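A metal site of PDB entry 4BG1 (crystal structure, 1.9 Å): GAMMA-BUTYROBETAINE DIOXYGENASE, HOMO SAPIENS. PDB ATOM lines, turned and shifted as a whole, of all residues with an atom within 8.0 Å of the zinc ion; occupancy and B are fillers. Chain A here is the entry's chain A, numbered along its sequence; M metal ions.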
ATOM      1  N   LEU A  34      19.263  18.616 -28.753  1.00  0.00           N
ATOM      2  CA  LEU A  34      20.159  18.486 -27.597  1.00  0.00           C
ATOM      3  C   LEU A  34      19.360  18.108 -26.338  1.00  0.00           C
ATOM      4  O   LEU A  34      19.690  17.164 -25.652  1.00  0.00           O
ATOM      5  CB  LEU A  34      20.929  19.785 -27.373  1.00  0.00           C
ATOM      6  CG  LEU A  34      22.001  20.120 -28.411  1.00  0.00           C
ATOM      7  CD1 LEU A  34      22.402  21.581 -28.232  1.00  0.00           C
ATOM      8  CD2 LEU A  34      23.220  19.224 -28.258  1.00  0.00           C
ATOM      9  N   ARG A  35      18.287  18.832 -26.062  1.00  0.00           N
ATOM     10  CA  ARG A  35      17.501  18.521 -24.880  1.00  0.00           C
ATOM     11  C   ARG A  35      16.961  17.077 -24.915  1.00  0.00           C
ATOM     12  O   ARG A  35      17.041  16.362 -23.911  1.00  0.00           O
ATOM     13  CB  ARG A  35      16.356  19.525 -24.687  1.00  0.00           C
ATOM     14  CG  ARG A  35      15.467  19.244 -23.482  1.00  0.00           C
ATOM     15  CD  ARG A  35      16.278  19.409 -22.176  1.00  0.00           C
ATOM     16  NE  ARG A  35      15.545  19.004 -20.966  1.00  0.00           N
ATOM     17  CZ  ARG A  35      15.577  17.781 -20.456  1.00  0.00           C
ATOM     18  NH1 ARG A  35      16.285  16.827 -21.072  1.00  0.00           N
ATOM     19  NH2 ARG A  35      14.925  17.502 -19.330  1.00  0.00           N
ATOM     20  N   ASP A  36      16.459  16.677 -26.085  1.00  0.00           N
ATOM     21  CA  ASP A  36      15.902  15.325 -26.358  1.00  0.00           C
ATOM     22  C   ASP A  36      16.942  14.240 -26.084  1.00  0.00           C
ATOM     23  O   ASP A  36      16.612  13.152 -25.636  1.00  0.00           O
ATOM     24  CB  ASP A  36      15.433  15.249 -27.819  1.00  0.00           C
ATOM     25  CG  ASP A  36      14.889  13.878 -28.199  1.00  0.00           C
ATOM     26  OD1 ASP A  36      14.015  13.390 -27.471  1.00  0.00           O
ATOM     27  OD2 ASP A  36      15.367  13.283 -29.183  1.00  0.00           O
ATOM     28  N   ASN A  37      18.216  14.596 -26.297  1.00  0.00           N
ATOM     29  CA  ASN A  37      19.300  13.648 -26.199  1.00  0.00           C
ATOM     30  C   ASN A  37      20.275  13.857 -25.045  1.00  0.00           C
ATOM     31  O   ASN A  37      21.412  13.387 -25.075  1.00  0.00           O
ATOM     32  CB  ASN A  37      19.995  13.548 -27.544  1.00  0.00           C
ATOM     33  CG  ASN A  37      19.093  12.879 -28.557  1.00  0.00           C
ATOM     34  OD1 ASN A  37      18.702  11.733 -28.348  1.00  0.00           O
ATOM     35  ND2 ASN A  37      18.671  13.614 -29.576  1.00  0.00           N
ATOM     36  N   CYS A  38      19.784  14.530 -24.006  1.00  0.00           N
ATOM     37  CA  CYS A  38      20.522  14.695 -22.759  1.00  0.00           C
ATOM     38  C   CYS A  38      20.944  13.324 -22.233  1.00  0.00           C
ATOM     39  O   CYS A  38      20.109  12.444 -22.098  1.00  0.00           O
ATOM     40  CB  CYS A  38      19.667  15.420 -21.714  1.00  0.00           C
ATOM     41  SG  CYS A  38      20.506  15.597 -20.098  1.00  0.00           S
ATOM     42  N   PRO A  39      22.229  13.122 -21.975  1.00  0.00           N
ATOM     43  CA  PRO A  39      22.684  11.807 -21.489  1.00  0.00           C
ATOM     44  C   PRO A  39      22.652  11.595 -19.987  1.00  0.00           C
ATOM     45  O   PRO A  39      23.211  10.592 -19.503  1.00  0.00           O
ATOM     46  CB  PRO A  39      24.144  11.719 -22.008  1.00  0.00           C
ATOM     47  CG  PRO A  39      24.585  13.135 -22.158  1.00  0.00           C
ATOM     48  CD  PRO A  39      23.351  13.990 -22.387  1.00  0.00           C
ATOM     49  N   CYS A  40      22.031  12.501 -19.227  1.00  0.00           N
ATOM     50  CA  CYS A  40      22.023  12.356 -17.763  1.00  0.00           C
ATOM     51  C   CYS A  40      21.127  11.191 -17.359  1.00  0.00           C
ATOM     52  O   CYS A  40      20.276  10.712 -18.136  1.00  0.00           O
ATOM     53  CB  CYS A  40      21.569  13.669 -17.061  1.00  0.00           C
ATOM     54  SG  CYS A  40      19.777  13.855 -16.842  1.00  0.00           S
ATOM     55  N   SER A  41      21.272  10.742 -16.117  1.00  0.00           N
ATOM     56  CA  SER A  41      20.571   9.525 -15.683  1.00  0.00           C
ATOM     57  C   SER A  41      19.062   9.735 -15.555  1.00  0.00           C
ATOM     58  O   SER A  41      18.320   8.753 -15.560  1.00  0.00           O
ATOM     59  CB  SER A  41      21.189   8.970 -14.390  1.00  0.00           C
ATOM     60  OG  SER A  41      20.954   9.859 -13.318  1.00  0.00           O
ATOM     61  N   ASP A  42      18.576  10.974 -15.457  1.00  0.00           N
ATOM     62  CA  ASP A  42      17.128  11.212 -15.503  1.00  0.00           C
ATOM     63  C   ASP A  42      16.557  10.950 -16.896  1.00  0.00           C
ATOM     64  O   ASP A  42      15.429  10.444 -17.022  1.00  0.00           O
ATOM     65  CB  ASP A  42      16.756  12.645 -15.129  1.00  0.00           C
ATOM     66  CG  ASP A  42      16.988  12.971 -13.656  1.00  0.00           C
ATOM     67  OD1 ASP A  42      17.314  12.087 -12.851  1.00  0.00           O
ATOM     68  OD2 ASP A  42      16.776  14.130 -13.300  1.00  0.00           O
ATOM     69  N   CYS A  43      17.343  11.269 -17.922  1.00  0.00           N
ATOM     70  CA  CYS A  43      16.881  11.302 -19.305  1.00  0.00           C
ATOM     71  C   CYS A  43      17.227  10.063 -20.100  1.00  0.00           C
ATOM     72  O   CYS A  43      16.657   9.845 -21.176  1.00  0.00           O
ATOM     73  CB  CYS A  43      17.527  12.503 -20.018  1.00  0.00           C
ATOM     74  SG  CYS A  43      16.926  14.087 -19.354  1.00  0.00           S
ATOM     75  N   TYR A  44      18.187   9.278 -19.603  1.00  0.00           N
ATOM     76  CA  TYR A  44      18.837   8.271 -20.386  1.00  0.00           C
ATOM     77  C   TYR A  44      19.237   7.114 -19.515  1.00  0.00           C
ATOM     78  O   TYR A  44      19.959   7.308 -18.513  1.00  0.00           O
ATOM     79  CB  TYR A  44      20.083   8.850 -21.027  1.00  0.00           C
ATOM     80  CG  TYR A  44      20.636   7.992 -22.099  1.00  0.00           C
ATOM     81  CD1 TYR A  44      20.082   8.013 -23.365  1.00  0.00           C
ATOM     82  CD2 TYR A  44      21.735   7.164 -21.866  1.00  0.00           C
ATOM     83  CE1 TYR A  44      20.584   7.230 -24.378  1.00  0.00           C
ATOM     84  CE2 TYR A  44      22.232   6.357 -22.877  1.00  0.00           C
ATOM     85  CZ  TYR A  44      21.656   6.410 -24.121  1.00  0.00           C
ATOM     86  OH  TYR A  44      22.110   5.629 -25.149  1.00  0.00           O
ATOM     87  N   LEU A  53      13.580   9.905 -21.331  1.00  0.00           N
ATOM     88  CA  LEU A  53      12.835  11.143 -21.494  1.00  0.00           C
ATOM     89  C   LEU A  53      11.616  10.950 -22.398  1.00  0.00           C
ATOM     90  O   LEU A  53      11.742  10.405 -23.483  1.00  0.00           O
ATOM     91  CB  LEU A  53      13.734  12.216 -22.121  1.00  0.00           C
ATOM     92  CG  LEU A  53      13.168  13.631 -22.212  1.00  0.00           C
ATOM     93  CD1 LEU A  53      13.164  14.314 -20.861  1.00  0.00           C
ATOM     94  CD2 LEU A  53      13.981  14.440 -23.233  1.00  0.00           C
ATOM     95  N   TRP A  78      19.306  24.644 -19.049  1.00  0.00           N
ATOM     96  CA  TRP A  78      18.033  24.846 -19.724  1.00  0.00           C
ATOM     97  C   TRP A  78      17.092  25.814 -18.964  1.00  0.00           C
ATOM     98  O   TRP A  78      17.228  26.009 -17.743  1.00  0.00           O
ATOM     99  CB  TRP A  78      17.380  23.471 -19.924  1.00  0.00           C
ATOM    100  CG  TRP A  78      18.182  22.534 -20.819  1.00  0.00           C
ATOM    101  CD1 TRP A  78      18.833  21.415 -20.429  1.00  0.00           C
ATOM    102  CD2 TRP A  78      18.385  22.650 -22.231  1.00  0.00           C
ATOM    103  NE1 TRP A  78      19.448  20.824 -21.498  1.00  0.00           N
ATOM    104  CE2 TRP A  78      19.189  21.560 -22.617  1.00  0.00           C
ATOM    105  CE3 TRP A  78      18.003  23.590 -23.189  1.00  0.00           C
ATOM    106  CZ2 TRP A  78      19.595  21.374 -23.942  1.00  0.00           C
ATOM    107  CZ3 TRP A  78      18.387  23.384 -24.507  1.00  0.00           C
ATOM    108  CH2 TRP A  78      19.164  22.286 -24.871  1.00  0.00           C
ATOM    109  N   HIS A  82      17.021  22.345 -15.790  1.00  0.00           N
ATOM    110  CA  HIS A  82      17.672  21.071 -16.138  1.00  0.00           C
ATOM    111  C   HIS A  82      19.092  21.332 -16.653  1.00  0.00           C
ATOM    112  O   HIS A  82      19.398  22.410 -17.212  1.00  0.00           O
ATOM    113  CB  HIS A  82      16.864  20.296 -17.201  1.00  0.00           C
ATOM    114  CG  HIS A  82      17.242  18.854 -17.259  1.00  0.00           C
ATOM    115  ND1 HIS A  82      16.800  17.940 -16.342  1.00  0.00           N
ATOM    116  CD2 HIS A  82      18.052  18.184 -18.106  1.00  0.00           C
ATOM    117  CE1 HIS A  82      17.302  16.760 -16.623  1.00  0.00           C
ATOM    118  NE2 HIS A  82      18.090  16.882 -17.679  1.00  0.00           N
ATOM    119  N   TYR A  83      19.976  20.357 -16.473  1.00  0.00           N
ATOM    120  CA  TYR A  83      21.388  20.571 -16.749  1.00  0.00           C
ATOM    121  C   TYR A  83      21.929  19.439 -17.581  1.00  0.00           C
ATOM    122  O   TYR A  83      21.654  18.290 -17.274  1.00  0.00           O
ATOM    123  CB  TYR A  83      22.171  20.669 -15.419  1.00  0.00           C
ATOM    124  CG  TYR A  83      23.651  20.621 -15.612  1.00  0.00           C
ATOM    125  CD1 TYR A  83      24.324  21.671 -16.229  1.00  0.00           C
ATOM    126  CD2 TYR A  83      24.405  19.516 -15.200  1.00  0.00           C
ATOM    127  CE1 TYR A  83      25.679  21.640 -16.421  1.00  0.00           C
ATOM    128  CE2 TYR A  83      25.782  19.475 -15.392  1.00  0.00           C
ATOM    129  CZ  TYR A  83      26.407  20.550 -16.003  1.00  0.00           C
ATOM    130  OH  TYR A  83      27.781  20.550 -16.222  1.00  0.00           O
ATOM    131  N   SER A  84      22.644  19.752 -18.674  1.00  0.00           N
ATOM    132  CA  SER A  84      23.181  18.721 -19.586  1.00  0.00           C
ATOM    133  C   SER A  84      24.660  18.879 -19.941  1.00  0.00           C
ATOM    134  O   SER A  84      25.132  19.998 -20.144  1.00  0.00           O
ATOM    135  CB  SER A  84      22.373  18.713 -20.909  1.00  0.00           C
ATOM    136  OG  SER A  84      20.964  18.518 -20.707  1.00  0.00           O
ATOM    137  N   GLU A  85      25.381  17.757 -20.059  1.00  0.00           N
ATOM    138  CA  GLU A  85      26.740  17.724 -20.607  1.00  0.00           C
ATOM    139  C   GLU A  85      26.823  16.895 -21.863  1.00  0.00           C
ATOM    140  O   GLU A  85      26.314  15.767 -21.899  1.00  0.00           O
ATOM    141  CB  GLU A  85      27.730  17.142 -19.581  1.00  0.00           C
ATOM    142  CG  GLU A  85      27.720  17.924 -18.273  1.00  0.00           C
ATOM    143  CD  GLU A  85      28.778  17.506 -17.261  1.00  0.00           C
ATOM    144  OE1 GLU A  85      29.539  16.554 -17.516  1.00  0.00           O
ATOM    145  OE2 GLU A  85      28.813  18.160 -16.187  1.00  0.00           O
ATOM    146  N   PHE A  86      27.514  17.413 -22.876  1.00  0.00           N
ATOM    147  CA  PHE A  86      27.753  16.663 -24.112  1.00  0.00           C
ATOM    148  C   PHE A  86      29.214  16.605 -24.491  1.00  0.00           C
ATOM    149  O   PHE A  86      29.909  17.624 -24.487  1.00  0.00           O
ATOM    150  CB  PHE A  86      26.994  17.311 -25.274  1.00  0.00           C
ATOM    151  CG  PHE A  86      25.524  17.452 -25.040  1.00  0.00           C
ATOM    152  CD1 PHE A  86      25.015  18.594 -24.439  1.00  0.00           C
ATOM    153  CD2 PHE A  86      24.648  16.450 -25.454  1.00  0.00           C
ATOM    154  CE1 PHE A  86      23.644  18.728 -24.220  1.00  0.00           C
ATOM    155  CE2 PHE A  86      23.285  16.590 -25.238  1.00  0.00           C
ATOM    156  CZ  PHE A  86      22.781  17.715 -24.624  1.00  0.00           C
HETATM  157 ZN    ZN M   1      18.919  15.088 -18.543  1.00  0.00          ZN
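SG of Cys 38 lies close to OG of Ser 84 (3.0 Å). The side-chain sulfur (SG) of Cys 43 lies close to the guanidinium group (NH1) of Arg 35 (3.3 Å). The side-chain sulfur of Cys 40 lies close to the backbone NH of Asp 42 (3.4 Å). O of Cys 43 sits at hydrogen-bond distance from N of Leu 53 (3.1 Å).
NE2 of His 82 is bound to the zinc ion (2.2 Å). SG of Cys 40 is bound to the zinc ion (2.3 Å). The zinc ion is bound by SG of Cys 38 (2.3 Å). SG of Cys 43 is bound to the zinc ion, at 2.4 Å.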
